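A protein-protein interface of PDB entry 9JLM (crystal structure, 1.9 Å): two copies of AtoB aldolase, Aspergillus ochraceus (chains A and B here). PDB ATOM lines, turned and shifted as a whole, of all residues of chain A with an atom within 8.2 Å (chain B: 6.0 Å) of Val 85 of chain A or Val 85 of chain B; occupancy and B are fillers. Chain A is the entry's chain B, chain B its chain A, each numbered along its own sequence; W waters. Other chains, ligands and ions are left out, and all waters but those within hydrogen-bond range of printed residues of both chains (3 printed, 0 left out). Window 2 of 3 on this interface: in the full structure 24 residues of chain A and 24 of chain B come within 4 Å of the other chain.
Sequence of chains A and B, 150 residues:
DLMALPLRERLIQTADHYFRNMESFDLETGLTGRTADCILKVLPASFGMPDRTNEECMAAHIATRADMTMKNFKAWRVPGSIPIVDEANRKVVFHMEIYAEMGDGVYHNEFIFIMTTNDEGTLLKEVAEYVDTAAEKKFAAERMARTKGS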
ATOM      1  N   PRO A   6     -14.509   9.926  -7.641  1.00  0.00           N
ATOM      2  CA  PRO A   6     -15.842   9.405  -7.329  1.00  0.00           C
ATOM      3  C   PRO A   6     -15.731   8.161  -6.452  1.00  0.00           C
ATOM      4  O   PRO A   6     -14.755   7.408  -6.523  1.00  0.00           O
ATOM      5  CB  PRO A   6     -16.433   9.087  -8.710  1.00  0.00           C
ATOM      6  CG  PRO A   6     -15.562   9.833  -9.696  1.00  0.00           C
ATOM      7  CD  PRO A   6     -14.209   9.861  -9.082  1.00  0.00           C
ATOM      8  N   LEU A   7     -16.743   7.962  -5.604  1.00  0.00           N
ATOM      9  CA  LEU A   7     -16.639   6.967  -4.541  1.00  0.00           C
ATOM     10  C   LEU A   7     -16.293   5.588  -5.099  1.00  0.00           C
ATOM     11  O   LEU A   7     -15.394   4.908  -4.584  1.00  0.00           O
ATOM     12  CB  LEU A   7     -17.936   6.925  -3.734  1.00  0.00           C
ATOM     13  CG  LEU A   7     -17.927   5.998  -2.515  1.00  0.00           C
ATOM     14  CD1 LEU A   7     -16.790   6.367  -1.590  1.00  0.00           C
ATOM     15  CD2 LEU A   7     -19.254   6.057  -1.787  1.00  0.00           C
ATOM     16  N   ARG A   8     -16.972   5.170  -6.169  1.00  0.00           N
ATOM     17  CA  ARG A   8     -16.705   3.852  -6.746  1.00  0.00           C
ATOM     18  C   ARG A   8     -15.225   3.682  -7.070  1.00  0.00           C
ATOM     19  O   ARG A   8     -14.577   2.731  -6.617  1.00  0.00           O
ATOM     20  CB  ARG A   8     -17.557   3.635  -8.005  1.00  0.00           C
ATOM     21  CG  ARG A   8     -17.293   2.283  -8.637  1.00  0.00           C
ATOM     22  CD  ARG A   8     -18.105   1.994  -9.886  1.00  0.00           C
ATOM     23  NE  ARG A   8     -18.083   0.560 -10.119  1.00  0.00           N
ATOM     24  CZ  ARG A   8     -19.066  -0.274  -9.794  1.00  0.00           C
ATOM     25  NH1 ARG A   8     -20.194   0.168  -9.253  1.00  0.00           N
ATOM     26  NH2 ARG A   8     -18.926  -1.558 -10.040  1.00  0.00           N
ATOM     27  N   GLU A   9     -14.668   4.618  -7.839  1.00  0.00           N
ATOM     28  CA  GLU A   9     -13.252   4.558  -8.181  1.00  0.00           C
ATOM     29  C   GLU A   9     -12.360   4.722  -6.952  1.00  0.00           C
ATOM     30  O   GLU A   9     -11.269   4.142  -6.897  1.00  0.00           O
ATOM     31  CB  GLU A   9     -12.930   5.628  -9.230  1.00  0.00           C
ATOM     32  CG  GLU A   9     -13.534   5.348 -10.619  1.00  0.00           C
ATOM     33  CD  GLU A   9     -15.069   5.335 -10.632  1.00  0.00           C
ATOM     34  OE1 GLU A   9     -15.685   6.171  -9.929  1.00  0.00           O
ATOM     35  OE2 GLU A   9     -15.658   4.469 -11.329  1.00  0.00           O
ATOM     36  N   ARG A  10     -12.787   5.516  -5.969  1.00  0.00           N
ATOM     37  CA  ARG A  10     -11.980   5.656  -4.759  1.00  0.00           C
ATOM     38  C   ARG A  10     -11.967   4.365  -3.949  1.00  0.00           C
ATOM     39  O   ARG A  10     -10.922   3.985  -3.396  1.00  0.00           O
ATOM     40  CB  ARG A  10     -12.477   6.823  -3.896  1.00  0.00           C
ATOM     41  CG  ARG A  10     -11.692   6.910  -2.590  1.00  0.00           C
ATOM     42  CD  ARG A  10     -11.855   8.201  -1.846  1.00  0.00           C
ATOM     43  NE  ARG A  10     -13.207   8.412  -1.362  1.00  0.00           N
ATOM     44  CZ  ARG A  10     -14.048   9.279  -1.897  1.00  0.00           C
ATOM     45  NH1 ARG A  10     -13.660  10.002  -2.937  1.00  0.00           N
ATOM     46  NH2 ARG A  10     -15.262   9.425  -1.390  1.00  0.00           N
ATOM     47  N   LEU A  11     -13.109   3.668  -3.879  1.00  0.00           N
ATOM     48  CA  LEU A  11     -13.146   2.380  -3.186  1.00  0.00           C
ATOM     49  C   LEU A  11     -12.229   1.362  -3.854  1.00  0.00           C
ATOM     50  O   LEU A  11     -11.513   0.618  -3.171  1.00  0.00           O
ATOM     51  CB  LEU A  11     -14.575   1.847  -3.118  1.00  0.00           C
ATOM     52  CG  LEU A  11     -15.571   2.634  -2.252  1.00  0.00           C
ATOM     53  CD1 LEU A  11     -17.000   2.093  -2.350  1.00  0.00           C
ATOM     54  CD2 LEU A  11     -15.107   2.685  -0.804  1.00  0.00           C
ATOM     55  N   ILE A  12     -12.230   1.308  -5.185  1.00  0.00           N
ATOM     56  CA  ILE A  12     -11.369   0.350  -5.875  1.00  0.00           C
ATOM     57  C   ILE A  12      -9.901   0.659  -5.592  1.00  0.00           C
ATOM     58  O   ILE A  12      -9.105  -0.246  -5.315  1.00  0.00           O
ATOM     59  CB  ILE A  12     -11.677   0.344  -7.391  1.00  0.00           C
ATOM     60  CG1 ILE A  12     -13.056  -0.264  -7.663  1.00  0.00           C
ATOM     61  CG2 ILE A  12     -10.623  -0.447  -8.169  1.00  0.00           C
ATOM     62  CD1 ILE A  12     -13.554  -0.056  -9.096  1.00  0.00           C
ATOM     63  N   GLN A  13      -9.522   1.942  -5.648  1.00  0.00           N
ATOM     64  CA  GLN A  13      -8.122   2.313  -5.437  1.00  0.00           C
ATOM     65  C   GLN A  13      -7.676   1.989  -4.019  1.00  0.00           C
ATOM     66  O   GLN A  13      -6.575   1.466  -3.813  1.00  0.00           O
ATOM     67  CB  GLN A  13      -7.902   3.798  -5.740  1.00  0.00           C
ATOM     68  CG  GLN A  13      -6.499   4.291  -5.353  1.00  0.00           C
ATOM     69  CD  GLN A  13      -6.041   5.513  -6.145  1.00  0.00           C
ATOM     70  OE1 GLN A  13      -6.615   5.854  -7.185  1.00  0.00           O
ATOM     71  NE2 GLN A  13      -4.992   6.172  -5.658  1.00  0.00           N
ATOM     72  N   ALA A  15      -9.067  -0.324  -2.058  1.00  0.00           N
ATOM     73  CA  ALA A  15      -9.016  -1.777  -1.974  1.00  0.00           C
ATOM     74  C   ALA A  15      -7.778  -2.315  -2.674  1.00  0.00           C
ATOM     75  O   ALA A  15      -7.055  -3.148  -2.126  1.00  0.00           O
ATOM     76  CB  ALA A  15     -10.291  -2.385  -2.570  1.00  0.00           C
ATOM     77  N   ILE A  82     -14.149  -8.405 -12.945  1.00  0.00           N
ATOM     78  CA  ILE A  82     -14.206  -6.976 -12.662  1.00  0.00           C
ATOM     79  C   ILE A  82     -14.398  -6.794 -11.161  1.00  0.00           C
ATOM     80  O   ILE A  82     -15.023  -7.642 -10.510  1.00  0.00           O
ATOM     81  CB  ILE A  82     -15.335  -6.293 -13.456  1.00  0.00           C
ATOM     82  CG1 ILE A  82     -16.650  -7.072 -13.305  1.00  0.00           C
ATOM     83  CG2 ILE A  82     -14.951  -6.153 -14.926  1.00  0.00           C
ATOM     84  CD1 ILE A  82     -17.544  -6.627 -12.121  1.00  0.00           C
ATOM     85  N   PRO A  83     -13.892  -5.718 -10.573  1.00  0.00           N
ATOM     86  CA  PRO A  83     -14.155  -5.482  -9.150  1.00  0.00           C
ATOM     87  C   PRO A  83     -15.646  -5.269  -8.914  1.00  0.00           C
ATOM     88  O   PRO A  83     -16.314  -4.542  -9.652  1.00  0.00           O
ATOM     89  CB  PRO A  83     -13.341  -4.216  -8.844  1.00  0.00           C
ATOM     90  CG  PRO A  83     -12.348  -4.113  -9.959  1.00  0.00           C
ATOM     91  CD  PRO A  83     -13.049  -4.665 -11.159  1.00  0.00           C
ATOM     92  N   ILE A  84     -16.161  -5.921  -7.881  1.00  0.00           N
ATOM     93  CA  ILE A  84     -17.545  -5.783  -7.463  1.00  0.00           C
ATOM     94  C   ILE A  84     -17.572  -4.764  -6.332  1.00  0.00           C
ATOM     95  O   ILE A  84     -16.975  -4.996  -5.277  1.00  0.00           O
ATOM     96  CB  ILE A  84     -18.112  -7.141  -7.020  1.00  0.00           C
ATOM     97  CG1 ILE A  84     -18.094  -8.119  -8.204  1.00  0.00           C
ATOM     98  CG2 ILE A  84     -19.509  -6.994  -6.416  1.00  0.00           C
ATOM     99  CD1 ILE A  84     -18.301  -9.574  -7.811  1.00  0.00           C
ATOM    100  N   VAL A  85     -18.237  -3.628  -6.548  1.00  0.00           N
ATOM    101  CA  VAL A  85     -18.212  -2.513  -5.598  1.00  0.00           C
ATOM    102  C   VAL A  85     -19.622  -2.240  -5.100  1.00  0.00           C
ATOM    103  O   VAL A  85     -20.528  -1.956  -5.896  1.00  0.00           O
ATOM    104  CB  VAL A  85     -17.613  -1.239  -6.215  1.00  0.00           C
ATOM    105  CG1 VAL A  85     -17.544  -0.131  -5.162  1.00  0.00           C
ATOM    106  CG2 VAL A  85     -16.238  -1.523  -6.804  1.00  0.00           C
ATOM    107  N   ASP A  86     -19.796  -2.294  -3.788  1.00  0.00           N
ATOM    108  CA  ASP A  86     -21.033  -1.922  -3.114  1.00  0.00           C
ATOM    109  C   ASP A  86     -20.760  -0.589  -2.413  1.00  0.00           C
ATOM    110  O   ASP A  86     -20.277  -0.551  -1.281  1.00  0.00           O
ATOM    111  CB  ASP A  86     -21.462  -3.017  -2.126  1.00  0.00           C
ATOM    112  CG  ASP A  86     -22.836  -2.785  -1.540  1.00  0.00           C
ATOM    113  OD1 ASP A  86     -23.335  -1.638  -1.558  1.00  0.00           O
ATOM    114  OD2 ASP A  86     -23.421  -3.761  -1.040  1.00  0.00           O
ATOM    115  N   GLU A  87     -21.082   0.507  -3.096  1.00  0.00           N
ATOM    116  CA  GLU A  87     -20.824   1.837  -2.543  1.00  0.00           C
ATOM    117  C   GLU A  87     -21.450   2.013  -1.166  1.00  0.00           C
ATOM    118  O   GLU A  87     -20.776   2.427  -0.218  1.00  0.00           O
ATOM    119  CB  GLU A  87     -21.351   2.909  -3.490  1.00  0.00           C
ATOM    120  CG  GLU A  87     -20.527   3.080  -4.730  1.00  0.00           C
ATOM    121  CD  GLU A  87     -20.997   4.263  -5.528  1.00  0.00           C
ATOM    122  OE1 GLU A  87     -21.548   5.202  -4.911  1.00  0.00           O
ATOM    123  OE2 GLU A  87     -20.840   4.244  -6.766  1.00  0.00           O
ATOM    124  N   ALA A  88     -22.747   1.723  -1.046  1.00  0.00           N
ATOM    125  CA  ALA A  88     -23.452   1.899   0.220  1.00  0.00           C
ATOM    126  C   ALA A  88     -22.733   1.202   1.366  1.00  0.00           C
ATOM    127  O   ALA A  88     -22.610   1.761   2.460  1.00  0.00           O
ATOM    128  CB  ALA A  88     -24.887   1.372   0.101  1.00  0.00           C
ATOM    129  N   ASN A  89     -22.244  -0.012   1.134  1.00  0.00           N
ATOM    130  CA  ASN A  89     -21.616  -0.803   2.183  1.00  0.00           C
ATOM    131  C   ASN A  89     -20.106  -0.620   2.252  1.00  0.00           C
ATOM    132  O   ASN A  89     -19.459  -1.279   3.080  1.00  0.00           O
ATOM    133  CB  ASN A  89     -21.938  -2.290   1.993  1.00  0.00           C
ATOM    134  CG  ASN A  89     -23.328  -2.652   2.490  1.00  0.00           C
ATOM    135  OD1 ASN A  89     -24.079  -3.368   1.822  1.00  0.00           O
ATOM    136  ND2 ASN A  89     -23.677  -2.157   3.665  1.00  0.00           N
ATOM    137  N   ARG A  90     -19.539   0.250   1.414  1.00  0.00           N
ATOM    138  CA  ARG A  90     -18.098   0.507   1.382  1.00  0.00           C
ATOM    139  C   ARG A  90     -17.312  -0.786   1.157  1.00  0.00           C
ATOM    140  O   ARG A  90     -16.234  -0.973   1.719  1.00  0.00           O
ATOM    141  CB  ARG A  90     -17.621   1.216   2.661  1.00  0.00           C
ATOM    142  CG  ARG A  90     -18.313   2.546   2.970  1.00  0.00           C
ATOM    143  CD  ARG A  90     -18.077   3.598   1.885  1.00  0.00           C
ATOM    144  NE  ARG A  90     -18.472   4.924   2.361  1.00  0.00           N
ATOM    145  CZ  ARG A  90     -19.699   5.431   2.260  1.00  0.00           C
ATOM    146  NH1 ARG A  90     -20.675   4.737   1.671  1.00  0.00           N
ATOM    147  NH2 ARG A  90     -19.954   6.640   2.753  1.00  0.00           N
ATOM    148  N   LYS A  91     -17.850  -1.670   0.314  1.00  0.00           N
ATOM    149  CA  LYS A  91     -17.305  -3.007   0.077  1.00  0.00           C
ATOM    150  C   LYS A  91     -16.791  -3.151  -1.355  1.00  0.00           C
ATOM    151  O   LYS A  91     -17.425  -2.678  -2.301  1.00  0.00           O
ATOM    152  CB  LYS A  91     -18.367  -4.082   0.329  1.00  0.00           C
ATOM    153  CG  LYS A  91     -18.652  -4.410   1.798  1.00  0.00           C
ATOM    154  CD  LYS A  91     -17.857  -5.640   2.252  1.00  0.00           C
ATOM    155  CE  LYS A  91     -18.350  -6.234   3.592  1.00  0.00           C
ATOM    156  NZ  LYS A  91     -18.127  -5.345   4.780  1.00  0.00           N
ATOM    157  N   VAL A  92     -15.642  -3.822  -1.510  1.00  0.00           N
ATOM    158  CA  VAL A  92     -15.102  -4.228  -2.809  1.00  0.00           C
ATOM    159  C   VAL A  92     -14.770  -5.721  -2.759  1.00  0.00           C
ATOM    160  O   VAL A  92     -14.191  -6.189  -1.771  1.00  0.00           O
ATOM    161  CB  VAL A  92     -13.839  -3.426  -3.176  1.00  0.00           C
ATOM    162  CG1 VAL A  92     -13.280  -3.900  -4.516  1.00  0.00           C
ATOM    163  CG2 VAL A  92     -14.133  -1.934  -3.207  1.00  0.00           C
ATOM    164  N   VAL A  93     -15.112  -6.462  -3.824  1.00  0.00           N
ATOM    165  CA  VAL A  93     -14.782  -7.885  -3.965  1.00  0.00           C
ATOM    166  C   VAL A  93     -13.922  -8.087  -5.209  1.00  0.00           C
ATOM    167  O   VAL A  93     -14.316  -7.686  -6.311  1.00  0.00           O
ATOM    168  CB  VAL A  93     -16.043  -8.762  -4.070  1.00  0.00           C
ATOM    169  CG1 VAL A  93     -15.658 -10.238  -4.055  1.00  0.00           C
ATOM    170  CG2 VAL A  93     -17.043  -8.415  -2.953  1.00  0.00           C
ATOM    171  N   PHE A  94     -12.767  -8.735  -5.040  1.00  0.00           N
ATOM    172  CA  PHE A  94     -11.907  -9.125  -6.153  1.00  0.00           C
ATOM    173  C   PHE A  94     -11.783 -10.645  -6.259  1.00  0.00           C
ATOM    174  O   PHE A  94     -11.768 -11.366  -5.252  1.00  0.00           O
ATOM    175  CB  PHE A  94     -10.468  -8.576  -6.022  1.00  0.00           C
ATOM    176  CG  PHE A  94     -10.364  -7.065  -5.974  1.00  0.00           C
ATOM    177  CD1 PHE A  94     -10.602  -6.301  -7.097  1.00  0.00           C
ATOM    178  CD2 PHE A  94      -9.979  -6.433  -4.809  1.00  0.00           C
ATOM    179  CE1 PHE A  94     -10.484  -4.917  -7.054  1.00  0.00           C
ATOM    180  CE2 PHE A  94      -9.859  -5.052  -4.757  1.00  0.00           C
ATOM    181  CZ  PHE A  94     -10.111  -4.292  -5.881  1.00  0.00           C
ATOM    182  N   MET A 115     -12.904  -6.473   0.607  1.00  0.00           N
ATOM    183  CA  MET A 115     -12.354  -5.316   1.295  1.00  0.00           C
ATOM    184  C   MET A 115     -13.487  -4.440   1.802  1.00  0.00           C
ATOM    185  O   MET A 115     -14.488  -4.255   1.109  1.00  0.00           O
ATOM    186  CB  MET A 115     -11.449  -4.494   0.369  1.00  0.00           C
ATOM    187  CG  MET A 115     -10.001  -4.971   0.313  1.00  0.00           C
ATOM    188  SD  MET A 115      -9.769  -6.489  -0.632  1.00  0.00           S
ATOM    189  CE  MET A 115      -8.004  -6.440  -0.891  1.00  0.00           C
ATOM    190  N   THR A 117     -13.847  -0.506   3.482  1.00  0.00           N
ATOM    191  CA  THR A 117     -13.111   0.702   3.790  1.00  0.00           C
ATOM    192  C   THR A 117     -13.799   1.436   4.928  1.00  0.00           C
ATOM    193  O   THR A 117     -14.858   1.033   5.410  1.00  0.00           O
ATOM    194  CB  THR A 117     -13.007   1.629   2.581  1.00  0.00           C
ATOM    195  OG1 THR A 117     -14.248   2.310   2.435  1.00  0.00           O
ATOM    196  CG2 THR A 117     -12.695   0.856   1.312  1.00  0.00           C
ATOM    197  N   LEU B   7     -33.817  -1.774  -7.269  1.00  0.00           N
ATOM    198  CA  LEU B   7     -32.894  -2.658  -7.978  1.00  0.00           C
ATOM    199  C   LEU B   7     -32.032  -3.450  -7.006  1.00  0.00           C
ATOM    200  O   LEU B   7     -31.844  -4.660  -7.178  1.00  0.00           O
ATOM    201  CB  LEU B   7     -32.012  -1.869  -8.942  1.00  0.00           C
ATOM    202  CG  LEU B   7     -31.015  -2.736  -9.726  1.00  0.00           C
ATOM    203  CD1 LEU B   7     -31.707  -3.859 -10.502  1.00  0.00           C
ATOM    204  CD2 LEU B   7     -30.152  -1.906 -10.657  1.00  0.00           C
ATOM    205  N   ARG B   8     -31.523  -2.788  -5.965  1.00  0.00           N
ATOM    206  CA  ARG B   8     -30.713  -3.476  -4.968  1.00  0.00           C
ATOM    207  C   ARG B   8     -31.442  -4.687  -4.387  1.00  0.00           C
ATOM    208  O   ARG B   8     -30.890  -5.797  -4.345  1.00  0.00           O
ATOM    209  CB  ARG B   8     -30.322  -2.498  -3.859  1.00  0.00           C
ATOM    210  CG  ARG B   8     -29.573  -3.149  -2.730  1.00  0.00           C
ATOM    211  CD  ARG B   8     -29.125  -2.144  -1.666  1.00  0.00           C
ATOM    212  NE  ARG B   8     -28.097  -2.767  -0.857  1.00  0.00           N
ATOM    213  CZ  ARG B   8     -26.799  -2.640  -1.094  1.00  0.00           C
ATOM    214  NH1 ARG B   8     -26.387  -1.870  -2.086  1.00  0.00           N
ATOM    215  NH2 ARG B   8     -25.919  -3.263  -0.323  1.00  0.00           N
ATOM    216  N   LEU B  11     -32.092  -7.522  -6.978  1.00  0.00           N
ATOM    217  CA  LEU B  11     -30.917  -8.364  -7.189  1.00  0.00           C
ATOM    218  C   LEU B  11     -30.759  -9.388  -6.076  1.00  0.00           C
ATOM    219  O   LEU B  11     -30.452 -10.558  -6.337  1.00  0.00           O
ATOM    220  CB  LEU B  11     -29.663  -7.490  -7.295  1.00  0.00           C
ATOM    221  CG  LEU B  11     -29.604  -6.616  -8.551  1.00  0.00           C
ATOM    222  CD1 LEU B  11     -28.475  -5.592  -8.513  1.00  0.00           C
ATOM    223  CD2 LEU B  11     -29.460  -7.505  -9.784  1.00  0.00           C
ATOM    224  N   ILE B  12     -30.961  -8.966  -4.824  1.00  0.00           N
ATOM    225  CA  ILE B  12     -30.854  -9.900  -3.704  1.00  0.00           C
ATOM    226  C   ILE B  12     -31.906 -10.998  -3.819  1.00  0.00           C
ATOM    227  O   ILE B  12     -31.597 -12.178  -3.643  1.00  0.00           O
ATOM    228  CB  ILE B  12     -30.955  -9.156  -2.359  1.00  0.00           C
ATOM    229  CG1 ILE B  12     -29.793  -8.171  -2.210  1.00  0.00           C
ATOM    230  CG2 ILE B  12     -30.978 -10.159  -1.201  1.00  0.00           C
ATOM    231  CD1 ILE B  12     -29.849  -7.338  -0.935  1.00  0.00           C
ATOM    232  N   PRO B  83     -25.436  -8.988   2.344  1.00  0.00           N
ATOM    233  CA  PRO B  83     -25.239  -9.139   0.898  1.00  0.00           C
ATOM    234  C   PRO B  83     -24.497  -7.935   0.326  1.00  0.00           C
ATOM    235  O   PRO B  83     -24.821  -6.782   0.626  1.00  0.00           O
ATOM    236  CB  PRO B  83     -26.672  -9.244   0.346  1.00  0.00           C
ATOM    237  CG  PRO B  83     -27.533  -9.572   1.519  1.00  0.00           C
ATOM    238  CD  PRO B  83     -26.862  -8.934   2.704  1.00  0.00           C
ATOM    239  N   ILE B  84     -23.490  -8.221  -0.495  1.00  0.00           N
ATOM    240  CA  ILE B  84     -22.722  -7.215  -1.217  1.00  0.00           C
ATOM    241  C   ILE B  84     -23.348  -7.065  -2.595  1.00  0.00           C
ATOM    242  O   ILE B  84     -23.317  -8.005  -3.399  1.00  0.00           O
ATOM    243  CB  ILE B  84     -21.240  -7.607  -1.323  1.00  0.00           C
ATOM    244  CG1 ILE B  84     -20.596  -7.652   0.068  1.00  0.00           C
ATOM    245  CG2 ILE B  84     -20.493  -6.646  -2.244  1.00  0.00           C
ATOM    246  CD1 ILE B  84     -19.154  -8.197   0.060  1.00  0.00           C
ATOM    247  N   VAL B  85     -23.905  -5.888  -2.887  1.00  0.00           N
ATOM    248  CA  VAL B  85     -24.624  -5.654  -4.139  1.00  0.00           C
ATOM    249  C   VAL B  85     -23.951  -4.545  -4.924  1.00  0.00           C
ATOM    250  O   VAL B  85     -23.766  -3.435  -4.410  1.00  0.00           O
ATOM    251  CB  VAL B  85     -26.103  -5.290  -3.916  1.00  0.00           C
ATOM    252  CG1 VAL B  85     -26.776  -5.142  -5.259  1.00  0.00           C
ATOM    253  CG2 VAL B  85     -26.806  -6.347  -3.096  1.00  0.00           C
ATOM    254  N   ASP B  86     -23.628  -4.840  -6.179  1.00  0.00           N
ATOM    255  CA  ASP B  86     -23.112  -3.882  -7.156  1.00  0.00           C
ATOM    256  C   ASP B  86     -24.203  -3.788  -8.226  1.00  0.00           C
ATOM    257  O   ASP B  86     -24.235  -4.568  -9.183  1.00  0.00           O
ATOM    258  CB  ASP B  86     -21.738  -4.345  -7.688  1.00  0.00           C
ATOM    259  CG  ASP B  86     -21.131  -3.405  -8.737  1.00  0.00           C
ATOM    260  OD1 ASP B  86     -21.819  -2.497  -9.252  1.00  0.00           O
ATOM    261  OD2 ASP B  86     -19.941  -3.605  -9.064  1.00  0.00           O
ATOM    262  N   GLU B  87     -25.121  -2.833  -8.023  1.00  0.00           N
ATOM    263  CA  GLU B  87     -26.261  -2.646  -8.918  1.00  0.00           C
ATOM    264  C   GLU B  87     -25.827  -2.449 -10.360  1.00  0.00           C
ATOM    265  O   GLU B  87     -26.446  -2.997 -11.281  1.00  0.00           O
ATOM    266  CB  GLU B  87     -27.080  -1.437  -8.479  1.00  0.00           C
ATOM    267  CG  GLU B  87     -27.805  -1.582  -7.189  1.00  0.00           C
ATOM    268  CD  GLU B  87     -28.529  -0.297  -6.816  1.00  0.00           C
ATOM    269  OE1 GLU B  87     -29.054   0.385  -7.722  1.00  0.00           O
ATOM    270  OE2 GLU B  87     -28.564   0.039  -5.618  1.00  0.00           O
ATOM    271  N   ASN B  89     -23.256  -3.473 -11.965  1.00  0.00           N
ATOM    272  CA  ASN B  89     -22.735  -4.702 -12.555  1.00  0.00           C
ATOM    273  C   ASN B  89     -23.679  -5.884 -12.393  1.00  0.00           C
ATOM    274  O   ASN B  89     -23.308  -6.998 -12.783  1.00  0.00           O
ATOM    275  CB  ASN B  89     -21.372  -5.057 -11.938  1.00  0.00           C
ATOM    276  CG  ASN B  89     -20.230  -4.250 -12.527  1.00  0.00           C
ATOM    277  OD1 ASN B  89     -20.211  -3.968 -13.725  1.00  0.00           O
ATOM    278  ND2 ASN B  89     -19.272  -3.872 -11.688  1.00  0.00           N
ATOM    279  N   LYS B  91     -24.454  -7.607  -9.830  1.00  0.00           N
ATOM    280  CA  LYS B  91     -23.754  -8.642  -9.081  1.00  0.00           C
ATOM    281  C   LYS B  91     -24.152  -8.617  -7.611  1.00  0.00           C
ATOM    282  O   LYS B  91     -24.347  -7.548  -7.031  1.00  0.00           O
ATOM    283  CB  LYS B  91     -22.238  -8.474  -9.215  1.00  0.00           C
ATOM    284  CG  LYS B  91     -21.740  -8.689 -10.641  1.00  0.00           C
ATOM    285  CD  LYS B  91     -20.523  -9.568 -10.690  1.00  0.00           C
ATOM    286  CE  LYS B  91     -19.935  -9.603 -12.097  1.00  0.00           C
ATOM    287  NZ  LYS B  91     -20.465 -10.710 -12.928  1.00  0.00           N
ATOM    288  N   VAL B  92     -24.266  -9.806  -7.012  1.00  0.00           N
ATOM    289  CA  VAL B  92     -24.525  -9.977  -5.585  1.00  0.00           C
ATOM    290  C   VAL B  92     -23.522 -10.995  -5.057  1.00  0.00           C
ATOM    291  O   VAL B  92     -23.275 -12.012  -5.713  1.00  0.00           O
ATOM    292  CB  VAL B  92     -25.968 -10.452  -5.326  1.00  0.00           C
ATOM    293  CG1 VAL B  92     -26.251 -10.594  -3.849  1.00  0.00           C
ATOM    294  CG2 VAL B  92     -26.968  -9.504  -5.980  1.00  0.00           C
ATOM    295  N   VAL B  93     -22.912 -10.699  -3.900  1.00  0.00           N
ATOM    296  CA  VAL B  93     -21.990 -11.616  -3.227  1.00  0.00           C
ATOM    297  C   VAL B  93     -22.566 -11.969  -1.860  1.00  0.00           C
ATOM    298  O   VAL B  93     -22.909 -11.078  -1.071  1.00  0.00           O
ATOM    299  CB  VAL B  93     -20.569 -11.029  -3.080  1.00  0.00           C
ATOM    300  CG1 VAL B  93     -19.605 -12.089  -2.582  1.00  0.00           C
ATOM    301  CG2 VAL B  93     -20.073 -10.462  -4.409  1.00  0.00           C
HETATM  302  O   HOH W   1     -22.617  -5.456   2.008  1.00  0.00           O
HETATM  303  O   HOH W   2     -27.022  -5.051   0.951  1.00  0.00           O
HETATM  304  O   HOH W   3     -23.532   0.370  -8.626  1.00  0.00           O
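The guanidinium group (NH2) of Arg 8 of chain B lies within salt-bridge range of the side-chain carboxylate (OD2) of Asp 86 of chain A, at 2.6 Å. The guanidinium group of Arg 8 of chain B sits at hydrogen-bond distance from the side-chain amide oxygen of Asn 89 of chain A (2.8 Å). The side-chain carboxylate (OD2) of Asp 86 of chain A is in hydrogen-bond range of the backbone NH (N) of Val 85 of chain B, at 2.9 Å. The guanidinium group (NH2) of Arg 8 of chain A lies within salt-bridge range of the side-chain carboxylate (OD2) of Asp 86 of chain B, at 2.5 Å. The backbone NH (N) of Val 85 of chain A is in hydrogen-bond range of the side-chain carboxylate (OD2) of Asp 86 of chain B (3.0 Å). NH2 of Arg 8 of chain A sits close to ND2 of Asn 89 of chain B (2.9 Å).
N of Asp 86 of chain B is in hydrogen-bond range of O of Lys 91 of chain B, 2.9 Å away. OD1 of Asp 86 of chain A sits close to N of Ala 88 of chain A (3.5 Å). The side-chain amide oxygen (OD1) of Asn 89 of chain A sits close to the side-chain carboxylate (OD2) of Asp 86 of chain A, at 3.0 Å.
OD2 of Asp 86 of chain B touches O of Pro 83 of chain A, 3.8 Å away. O of Pro 83 of chain A touches ND2 of Asn 89 of chain B (3.7 Å). CD1 of Ile 84 of chain A touches CD of Lys 91 of chain B (3.6 Å). O of Pro 83 of chain B touches OD2 of Asp 86 of chain A, at 3.7 Å. OD1 of Asn 89 of chain A touches O of Pro 83 of chain B (3.7 Å). Val 93 of chain B touches Val 93 of chain A (CG2 to CG2, 3.9 Å).
Of chain B, only Val 85 (3.9 Å) and Asp 86 (3.0 Å) come within 4 Å of Val 85 of chain A. Val 85 of chain B touches two residues of chain A. Of the printed residues of chain A, Val 93 of chain B touches Ile 84 and Val 93. Printed residues of chain A within 4 Å of Arg 8 of chain B: Asp 86 (2.6 Å) and Asn 89 (2.8 Å). The nearest residue of chain B that does not touch Val 85 of chain A is Glu 87 of chain B (5.1 Å). The nearest residue of chain A that does not touch Val 85 of chain B is Glu 87 of chain A (4.9 Å).
Printed residues of chain B that touch a printed residue of chain A: Arg 8, Pro 83, Ile 84, Val 85, Asp 86, Asn 89, Lys 91 and Val 93. Hydrophobic or aromatic side chains of chain B within 4 Å of the printed part of chain A: Ile 84 and Val 93. Of the 24 printed residues of chain A, 9 touch a printed residue of chain B. Among the printed residues, Asp or Glu carboxylates within 4 Å of a Lys or Arg side-chain nitrogen of the other chain: Arg 8 of chain A with Asp 86 of chain B and Asp 86 of chain A with Arg 8 of chain B.
Pro 83 of chain A touches Asp 86 of chain B, and with the chains exchanged Asp 86 of chain A touches Pro 83 of chain B. Val 85 of chain A touches its own counterpart, Val 85 of chain B. Val 93 of chain A touches its own counterpart, Val 93 of chain B. Positions printed for both chains: 7, 8, 11, 12, 83, 84, 85, 86, 87, 89, 91, 92 and 93.
Water W1 bridges OD1 of Asn 89 of chain A and O of Pro 83 of chain B. Water W3 lies within hydrogen-bond range of OD1 of Asp 86 of chain B and NH1 of Arg 8 of chain A.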
